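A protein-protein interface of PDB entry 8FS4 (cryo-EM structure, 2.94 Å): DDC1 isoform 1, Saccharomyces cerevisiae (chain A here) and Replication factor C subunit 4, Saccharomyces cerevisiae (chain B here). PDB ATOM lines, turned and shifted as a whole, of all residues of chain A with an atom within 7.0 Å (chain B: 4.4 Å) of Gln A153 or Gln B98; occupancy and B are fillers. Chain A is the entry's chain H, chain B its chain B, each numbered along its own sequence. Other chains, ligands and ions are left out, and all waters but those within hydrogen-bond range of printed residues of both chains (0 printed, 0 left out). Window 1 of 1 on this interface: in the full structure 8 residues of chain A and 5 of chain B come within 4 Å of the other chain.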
ATOM      1  N   ASP A  28      31.486  -7.883 -20.674  1.00  0.00           N
ATOM      2  CA  ASP A  28      30.166  -7.307 -20.433  1.00  0.00           C
ATOM      3  C   ASP A  28      30.109  -6.602 -19.083  1.00  0.00           C
ATOM      4  O   ASP A  28      29.550  -5.504 -18.972  1.00  0.00           O
ATOM      5  CB  ASP A  28      29.094  -8.393 -20.517  1.00  0.00           C
ATOM      6  CG  ASP A  28      29.351  -9.544 -19.565  1.00  0.00           C
ATOM      7  OD1 ASP A  28      30.523  -9.761 -19.194  1.00  0.00           O
ATOM      8  OD2 ASP A  28      28.380 -10.233 -19.188  1.00  0.00           O
ATOM      9  N   ASP A  29      30.678  -7.214 -18.047  1.00  0.00           N
ATOM     10  CA  ASP A  29      30.714  -6.632 -16.710  1.00  0.00           C
ATOM     11  C   ASP A  29      32.121  -6.104 -16.455  1.00  0.00           C
ATOM     12  O   ASP A  29      33.067  -6.885 -16.310  1.00  0.00           O
ATOM     13  CB  ASP A  29      30.316  -7.662 -15.656  1.00  0.00           C
ATOM     14  CG  ASP A  29      29.191  -8.564 -16.118  1.00  0.00           C
ATOM     15  OD1 ASP A  29      28.018  -8.140 -16.044  1.00  0.00           O
ATOM     16  OD2 ASP A  29      29.479  -9.697 -16.557  1.00  0.00           O
ATOM     17  N   LYS A  31      35.113  -4.497 -14.324  1.00  0.00           N
ATOM     18  CA  LYS A  31      35.539  -4.766 -12.961  1.00  0.00           C
ATOM     19  C   LYS A  31      36.356  -3.582 -12.463  1.00  0.00           C
ATOM     20  O   LYS A  31      37.317  -3.168 -13.119  1.00  0.00           O
ATOM     21  CB  LYS A  31      36.355  -6.053 -12.906  1.00  0.00           C
ATOM     22  CG  LYS A  31      36.166  -6.847 -11.639  1.00  0.00           C
ATOM     23  CD  LYS A  31      37.285  -7.842 -11.393  1.00  0.00           C
ATOM     24  CE  LYS A  31      37.859  -8.501 -12.658  1.00  0.00           C
ATOM     25  NZ  LYS A  31      37.033  -9.647 -13.113  1.00  0.00           N
ATOM     26  N   GLY A  77      34.021  -8.996  -0.989  1.00  0.00           N
ATOM     27  CA  GLY A  77      34.053  -7.548  -0.907  1.00  0.00           C
ATOM     28  C   GLY A  77      35.408  -7.018  -0.480  1.00  0.00           C
ATOM     29  O   GLY A  77      36.327  -6.910  -1.292  1.00  0.00           O
ATOM     30  N   TYR A  92      38.581  -2.856  -1.732  1.00  0.00           N
ATOM     31  CA  TYR A  92      37.225  -3.341  -2.098  1.00  0.00           C
ATOM     32  C   TYR A  92      37.192  -3.640  -3.600  1.00  0.00           C
ATOM     33  O   TYR A  92      37.576  -2.758  -4.391  1.00  0.00           O
ATOM     34  CB  TYR A  92      36.152  -2.307  -1.753  1.00  0.00           C
ATOM     35  CG  TYR A  92      34.745  -2.834  -1.875  1.00  0.00           C
ATOM     36  CD1 TYR A  92      34.288  -3.834  -1.036  1.00  0.00           C
ATOM     37  CD2 TYR A  92      33.885  -2.359  -2.850  1.00  0.00           C
ATOM     38  CE1 TYR A  92      33.001  -4.333  -1.142  1.00  0.00           C
ATOM     39  CE2 TYR A  92      32.596  -2.851  -2.973  1.00  0.00           C
ATOM     40  CZ  TYR A  92      32.152  -3.841  -2.116  1.00  0.00           C
ATOM     41  OH  TYR A  92      30.877  -4.341  -2.222  1.00  0.00           O
ATOM     42  N   SER A  93      36.750  -4.843  -3.978  1.00  0.00           N
ATOM     43  CA  SER A  93      36.636  -5.199  -5.418  1.00  0.00           C
ATOM     44  C   SER A  93      35.169  -5.473  -5.755  1.00  0.00           C
ATOM     45  O   SER A  93      34.489  -6.113  -4.930  1.00  0.00           O
ATOM     46  CB  SER A  93      37.509  -6.375  -5.760  1.00  0.00           C
ATOM     47  OG  SER A  93      37.217  -6.857  -7.063  1.00  0.00           O
ATOM     48  N   PHE A  94      34.701  -5.002  -6.914  1.00  0.00           N
ATOM     49  CA  PHE A  94      33.261  -5.162  -7.247  1.00  0.00           C
ATOM     50  C   PHE A  94      33.054  -5.259  -8.761  1.00  0.00           C
ATOM     51  O   PHE A  94      33.926  -4.787  -9.518  1.00  0.00           O
ATOM     52  CB  PHE A  94      32.441  -4.030  -6.617  1.00  0.00           C
ATOM     53  CG  PHE A  94      32.726  -2.645  -7.138  1.00  0.00           C
ATOM     54  CD1 PHE A  94      32.316  -2.256  -8.403  1.00  0.00           C
ATOM     55  CD2 PHE A  94      33.414  -1.726  -6.362  1.00  0.00           C
ATOM     56  CE1 PHE A  94      32.579  -0.982  -8.877  1.00  0.00           C
ATOM     57  CE2 PHE A  94      33.679  -0.452  -6.837  1.00  0.00           C
ATOM     58  CZ  PHE A  94      33.261  -0.082  -8.093  1.00  0.00           C
ATOM     59  N   ARG A  95      31.939  -5.860  -9.180  1.00  0.00           N
ATOM     60  CA  ARG A  95      31.601  -5.995 -10.591  1.00  0.00           C
ATOM     61  C   ARG A  95      30.346  -5.185 -10.886  1.00  0.00           C
ATOM     62  O   ARG A  95      29.383  -5.217 -10.113  1.00  0.00           O
ATOM     63  CB  ARG A  95      31.366  -7.464 -10.951  1.00  0.00           C
ATOM     64  CG  ARG A  95      32.121  -7.956 -12.172  1.00  0.00           C
ATOM     65  CD  ARG A  95      31.550  -9.280 -12.663  1.00  0.00           C
ATOM     66  NE  ARG A  95      31.225 -10.178 -11.560  1.00  0.00           N
ATOM     67  CZ  ARG A  95      29.997 -10.496 -11.168  1.00  0.00           C
ATOM     68  NH1 ARG A  95      28.923 -10.002 -11.765  1.00  0.00           N
ATOM     69  NH2 ARG A  95      29.840 -11.331 -10.143  1.00  0.00           N
ATOM     70  N   VAL A  96      30.354  -4.459 -12.005  1.00  0.00           N
ATOM     71  CA  VAL A  96      29.188  -3.712 -12.459  1.00  0.00           C
ATOM     72  C   VAL A  96      29.113  -3.806 -13.977  1.00  0.00           C
ATOM     73  O   VAL A  96      30.135  -3.904 -14.664  1.00  0.00           O
ATOM     74  CB  VAL A  96      29.223  -2.235 -11.996  1.00  0.00           C
ATOM     75  CG1 VAL A  96      30.363  -1.478 -12.663  1.00  0.00           C
ATOM     76  CG2 VAL A  96      27.889  -1.556 -12.271  1.00  0.00           C
ATOM     77  N   ASN A  97      27.889  -3.777 -14.501  1.00  0.00           N
ATOM     78  CA  ASN A  97      27.685  -3.967 -15.931  1.00  0.00           C
ATOM     79  C   ASN A  97      28.366  -2.861 -16.728  1.00  0.00           C
ATOM     80  O   ASN A  97      28.182  -1.672 -16.450  1.00  0.00           O
ATOM     81  CB  ASN A  97      26.192  -4.001 -16.251  1.00  0.00           C
ATOM     82  CG  ASN A  97      25.907  -4.561 -17.629  1.00  0.00           C
ATOM     83  OD1 ASN A  97      26.824  -4.827 -18.404  1.00  0.00           O
ATOM     84  ND2 ASN A  97      24.630  -4.744 -17.942  1.00  0.00           N
ATOM     85  N   ASN A 132      22.836  -2.173  -1.905  1.00  0.00           N
ATOM     86  CA  ASN A 132      23.986  -2.791  -2.552  1.00  0.00           C
ATOM     87  C   ASN A 132      24.023  -2.450  -4.038  1.00  0.00           C
ATOM     88  O   ASN A 132      24.143  -3.337  -4.883  1.00  0.00           O
ATOM     89  CB  ASN A 132      23.958  -4.310  -2.361  1.00  0.00           C
ATOM     90  CG  ASN A 132      22.629  -4.923  -2.757  1.00  0.00           C
ATOM     91  OD1 ASN A 132      21.904  -4.380  -3.591  1.00  0.00           O
ATOM     92  ND2 ASN A 132      22.301  -6.060  -2.156  1.00  0.00           N
ATOM     93  N   GLN A 151      23.468  -1.514 -10.021  1.00  0.00           N
ATOM     94  CA  GLN A 151      23.778  -2.565  -9.063  1.00  0.00           C
ATOM     95  C   GLN A 151      25.194  -3.086  -9.274  1.00  0.00           C
ATOM     96  O   GLN A 151      25.677  -3.174 -10.406  1.00  0.00           O
ATOM     97  CB  GLN A 151      22.777  -3.714  -9.187  1.00  0.00           C
ATOM     98  CG  GLN A 151      22.592  -4.222 -10.604  1.00  0.00           C
ATOM     99  CD  GLN A 151      21.962  -5.596 -10.651  1.00  0.00           C
ATOM    100  OE1 GLN A 151      22.633  -6.591 -10.930  1.00  0.00           O
ATOM    101  NE2 GLN A 151      20.664  -5.661 -10.380  1.00  0.00           N
ATOM    102  N   PHE A 152      25.854  -3.441  -8.173  1.00  0.00           N
ATOM    103  CA  PHE A 152      27.225  -3.927  -8.196  1.00  0.00           C
ATOM    104  C   PHE A 152      27.340  -5.168  -7.321  1.00  0.00           C
ATOM    105  O   PHE A 152      26.578  -5.348  -6.368  1.00  0.00           O
ATOM    106  CB  PHE A 152      28.215  -2.844  -7.723  1.00  0.00           C
ATOM    107  CG  PHE A 152      28.254  -2.653  -6.230  1.00  0.00           C
ATOM    108  CD1 PHE A 152      27.088  -2.569  -5.490  1.00  0.00           C
ATOM    109  CD2 PHE A 152      29.464  -2.550  -5.567  1.00  0.00           C
ATOM    110  CE1 PHE A 152      27.134  -2.392  -4.121  1.00  0.00           C
ATOM    111  CE2 PHE A 152      29.509  -2.374  -4.199  1.00  0.00           C
ATOM    112  CZ  PHE A 152      28.341  -2.295  -3.478  1.00  0.00           C
ATOM    113  N   GLN A 153      28.303  -6.026  -7.658  1.00  0.00           N
ATOM    114  CA  GLN A 153      28.482  -7.314  -6.994  1.00  0.00           C
ATOM    115  C   GLN A 153      29.882  -7.408  -6.400  1.00  0.00           C
ATOM    116  O   GLN A 153      30.868  -7.377  -7.157  1.00  0.00           O
ATOM    117  CB  GLN A 153      28.249  -8.458  -7.982  1.00  0.00           C
ATOM    118  CG  GLN A 153      26.806  -8.598  -8.432  1.00  0.00           C
ATOM    119  CD  GLN A 153      26.519  -7.846  -9.718  1.00  0.00           C
ATOM    120  OE1 GLN A 153      27.358  -7.788 -10.617  1.00  0.00           O
ATOM    121  NE2 GLN A 153      25.326  -7.269  -9.812  1.00  0.00           N
ATOM    122  N   PRO A 154      30.040  -7.520  -5.079  1.00  0.00           N
ATOM    123  CA  PRO A 154      31.389  -7.654  -4.513  1.00  0.00           C
ATOM    124  C   PRO A 154      32.078  -8.927  -4.984  1.00  0.00           C
ATOM    125  O   PRO A 154      31.466  -9.993  -5.073  1.00  0.00           O
ATOM    126  CB  PRO A 154      31.145  -7.671  -2.999  1.00  0.00           C
ATOM    127  CG  PRO A 154      29.699  -7.972  -2.825  1.00  0.00           C
ATOM    128  CD  PRO A 154      29.006  -7.445  -4.032  1.00  0.00           C
ATOM    129  N   ILE A 155      33.372  -8.803  -5.284  1.00  0.00           N
ATOM    130  CA  ILE A 155      34.201  -9.933  -5.699  1.00  0.00           C
ATOM    131  C   ILE A 155      35.621  -9.714  -5.191  1.00  0.00           C
ATOM    132  O   ILE A 155      35.905  -8.709  -4.530  1.00  0.00           O
ATOM    133  CB  ILE A 155      34.175 -10.120  -7.226  1.00  0.00           C
ATOM    134  CG1 ILE A 155      34.091  -8.763  -7.927  1.00  0.00           C
ATOM    135  CG2 ILE A 155      33.006 -11.007  -7.626  1.00  0.00           C
ATOM    136  CD1 ILE A 155      34.246  -8.842  -9.426  1.00  0.00           C
ATOM    137  N   LYS A 156      36.521 -10.648  -5.491  1.00  0.00           N
ATOM    138  CA  LYS A 156      37.896 -10.595  -5.016  1.00  0.00           C
ATOM    139  C   LYS A 156      38.850 -10.151  -6.120  1.00  0.00           C
ATOM    140  O   LYS A 156      38.623 -10.402  -7.307  1.00  0.00           O
ATOM    141  CB  LYS A 156      38.336 -11.961  -4.478  1.00  0.00           C
ATOM    142  CG  LYS A 156      37.781 -12.330  -3.099  1.00  0.00           C
ATOM    143  CD  LYS A 156      37.848 -11.171  -2.112  1.00  0.00           C
ATOM    144  CE  LYS A 156      37.511 -11.610  -0.699  1.00  0.00           C
ATOM    145  NZ  LYS A 156      38.563 -12.486  -0.116  1.00  0.00           N
ATOM    146  N   LYS B  94      18.627 -12.325 -16.873  1.00  0.00           N
ATOM    147  CA  LYS B  94      20.013 -12.468 -16.448  1.00  0.00           C
ATOM    148  C   LYS B  94      20.401 -11.419 -15.414  1.00  0.00           C
ATOM    149  O   LYS B  94      21.051 -11.751 -14.415  1.00  0.00           O
ATOM    150  CB  LYS B  94      20.949 -12.383 -17.655  1.00  0.00           C
ATOM    151  CG  LYS B  94      22.422 -12.548 -17.314  1.00  0.00           C
ATOM    152  CD  LYS B  94      23.277 -12.531 -18.568  1.00  0.00           C
ATOM    153  CE  LYS B  94      24.758 -12.411 -18.241  1.00  0.00           C
ATOM    154  NZ  LYS B  94      25.099 -11.105 -17.610  1.00  0.00           N
ATOM    155  N   HIS B  95      20.013 -10.156 -15.617  1.00  0.00           N
ATOM    156  CA  HIS B  95      20.334  -9.144 -14.618  1.00  0.00           C
ATOM    157  C   HIS B  95      19.594  -9.409 -13.314  1.00  0.00           C
ATOM    158  O   HIS B  95      20.131  -9.164 -12.228  1.00  0.00           O
ATOM    159  CB  HIS B  95      20.012  -7.753 -15.156  1.00  0.00           C
ATOM    160  CG  HIS B  95      20.890  -7.335 -16.292  1.00  0.00           C
ATOM    161  ND1 HIS B  95      22.105  -7.932 -16.550  1.00  0.00           N
ATOM    162  CD2 HIS B  95      20.732  -6.382 -17.240  1.00  0.00           C
ATOM    163  CE1 HIS B  95      22.658  -7.364 -17.607  1.00  0.00           C
ATOM    164  NE2 HIS B  95      21.845  -6.420 -18.045  1.00  0.00           N
ATOM    165  N   PHE B  96      18.361  -9.910 -13.399  1.00  0.00           N
ATOM    166  CA  PHE B  96      17.619 -10.245 -12.190  1.00  0.00           C
ATOM    167  C   PHE B  96      18.305 -11.360 -11.413  1.00  0.00           C
ATOM    168  O   PHE B  96      18.371 -11.316 -10.179  1.00  0.00           O
ATOM    169  CB  PHE B  96      16.189 -10.640 -12.548  1.00  0.00           C
ATOM    170  CG  PHE B  96      15.342 -10.994 -11.363  1.00  0.00           C
ATOM    171  CD1 PHE B  96      14.848 -10.009 -10.529  1.00  0.00           C
ATOM    172  CD2 PHE B  96      15.031 -12.312 -11.087  1.00  0.00           C
ATOM    173  CE1 PHE B  96      14.067 -10.335  -9.442  1.00  0.00           C
ATOM    174  CE2 PHE B  96      14.251 -12.640 -10.002  1.00  0.00           C
ATOM    175  CZ  PHE B  96      13.768 -11.651  -9.180  1.00  0.00           C
ATOM    176  N   ALA B  97      18.818 -12.372 -12.114  1.00  0.00           N
ATOM    177  CA  ALA B  97      19.523 -13.451 -11.431  1.00  0.00           C
ATOM    178  C   ALA B  97      20.835 -12.961 -10.833  1.00  0.00           C
ATOM    179  O   ALA B  97      21.200 -13.353  -9.719  1.00  0.00           O
ATOM    180  CB  ALA B  97      19.773 -14.607 -12.395  1.00  0.00           C
ATOM    181  N   GLN B  98      21.561 -12.104 -11.554  1.00  0.00           N
ATOM    182  CA  GLN B  98      22.834 -11.610 -11.041  1.00  0.00           C
ATOM    183  C   GLN B  98      22.655 -10.644  -9.876  1.00  0.00           C
ATOM    184  O   GLN B  98      23.629 -10.356  -9.171  1.00  0.00           O
ATOM    185  CB  GLN B  98      23.622 -10.929 -12.158  1.00  0.00           C
ATOM    186  CG  GLN B  98      24.658 -11.822 -12.808  1.00  0.00           C
ATOM    187  CD  GLN B  98      25.292 -11.182 -14.024  1.00  0.00           C
ATOM    188  OE1 GLN B  98      25.044 -10.016 -14.324  1.00  0.00           O
ATOM    189  NE2 GLN B  98      26.121 -11.944 -14.728  1.00  0.00           N
ATOM    190  N   LYS B  99      21.444 -10.141  -9.662  1.00  0.00           N
ATOM    191  CA  LYS B  99      21.193  -9.218  -8.563  1.00  0.00           C
ATOM    192  C   LYS B  99      21.364  -9.928  -7.226  1.00  0.00           C
ATOM    193  O   LYS B  99      20.906 -11.062  -7.051  1.00  0.00           O
ATOM    194  CB  LYS B  99      19.783  -8.647  -8.683  1.00  0.00           C
ATOM    195  CG  LYS B  99      19.446  -7.587  -7.653  1.00  0.00           C
ATOM    196  CD  LYS B  99      18.047  -7.026  -7.859  1.00  0.00           C
ATOM    197  CE  LYS B  99      16.970  -8.089  -7.697  1.00  0.00           C
ATOM    198  NZ  LYS B  99      15.606  -7.537  -7.913  1.00  0.00           N
ATOM    199  N   LYS B 100      22.020  -9.260  -6.281  1.00  0.00           N
ATOM    200  CA  LYS B 100      22.199  -9.783  -4.932  1.00  0.00           C
ATOM    201  C   LYS B 100      21.225  -9.077  -3.999  1.00  0.00           C
ATOM    202  O   LYS B 100      21.253  -7.848  -3.878  1.00  0.00           O
ATOM    203  CB  LYS B 100      23.634  -9.589  -4.444  1.00  0.00           C
ATOM    204  CG  LYS B 100      24.662  -9.433  -5.552  1.00  0.00           C
ATOM    205  CD  LYS B 100      26.085  -9.500  -5.013  1.00  0.00           C
ATOM    206  CE  LYS B 100      26.405 -10.862  -4.413  1.00  0.00           C
ATOM    207  NZ  LYS B 100      27.806 -11.283  -4.688  1.00  0.00           N
ATOM    208  N   TYR B 134      23.110 -19.680 -12.302  1.00  0.00           N
ATOM    209  CA  TYR B 134      22.563 -18.947 -11.164  1.00  0.00           C
ATOM    210  C   TYR B 134      21.532 -19.772 -10.405  1.00  0.00           C
ATOM    211  O   TYR B 134      20.455 -19.284 -10.059  1.00  0.00           O
ATOM    212  CB  TYR B 134      21.934 -17.631 -11.617  1.00  0.00           C
ATOM    213  CG  TYR B 134      22.767 -16.852 -12.600  1.00  0.00           C
ATOM    214  CD1 TYR B 134      24.070 -16.488 -12.301  1.00  0.00           C
ATOM    215  CD2 TYR B 134      22.251 -16.482 -13.832  1.00  0.00           C
ATOM    216  CE1 TYR B 134      24.832 -15.774 -13.197  1.00  0.00           C
ATOM    217  CE2 TYR B 134      23.006 -15.771 -14.736  1.00  0.00           C
ATOM    218  CZ  TYR B 134      24.296 -15.420 -14.416  1.00  0.00           C
ATOM    219  OH  TYR B 134      25.054 -14.710 -15.316  1.00  0.00           O
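The side-chain carboxylate of Asp A28 is in salt-bridge range of the side-chain amino group of Lys B94, 3.7 Å away.
A ring nitrogen (NE2) of His B95 sits at hydrogen-bond distance from the side-chain amide nitrogen (ND2) of Asn A97 (3.3 Å).
The backbone carbonyl oxygen of Lys B100 sits at hydrogen-bond distance from the side-chain amide nitrogen of Asn A132, at 2.7 Å.
The side-chain amide nitrogen (NE2) of Gln B98 lies close to the side-chain amino group (NZ) of Lys B94 (3.2 Å).
The side-chain hydroxyl (OH) of Tyr B134 lies within hydrogen-bond range of the side-chain amide nitrogen (NE2) of Gln B98, 3.0 Å away.
The backbone carbonyl oxygen of Asp A28 lies close to the side-chain amide oxygen of Asn A97 (2.9 Å).
N of Arg A95 lies within hydrogen-bond range of O of Gln A153 (2.7 Å).
The side-chain amide nitrogen (NE2) of Gln A153 is in hydrogen-bond range of the side-chain amide oxygen (OE1) of Gln A151, at 3.0 Å.
Among the printed residues, pairs that only touch across the chains: Asp A29 with Gln B98, Gln A151 with His B95, Gln A151 with Lys B99, Gln A153 with Gln B98, Gln A153 with Lys B100 and Pro A154 with Lys B100.
Gln A153 touches just these residues of chain B: Gln B98 (3.6 Å) and Lys B100 (3.6 Å).
Gln B98 touches two residues of chain A.
Printed residues of chain B within 4 Å of Asp A29: Gln B98 (3.9 Å).
Printed residues of chain B within 4 Å of Pro A154: Lys B100.
Of the printed residues of chain A, Lys B94 touches Asp A28.
Printed residues of chain B within 4 Å of Asn A97: His B95 (3.3 Å).
The nearest residue of chain A that does not touch Gln B98 is Gln A151 (4.2 Å).
The nearest printed residue of chain B that does not touch Gln A151 is Gln B98 (4.2 Å).
Hydrophobic or aromatic side chains of chain B that line the printed part of chain A: His B95.
Of the 17 printed residues of chain A, 7 touch a printed residue of chain B.
Printed residues of chain A that touch a printed residue of chain B: Asp A28, Asp A29, Asn A97, Asn A132, Gln A151, Gln A153 and Pro A154.
Hydrophobic or aromatic side chains of chain A within 4 Å of the printed part of chain B: Pro A154.
Among the printed residues, 9 pairs touch across the chains.
Among the printed residues, Asp or Glu carboxylates within 4 Å of a Lys or Arg side-chain nitrogen of the other chain: Asp A28 with Lys B94 (3.7 Å).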
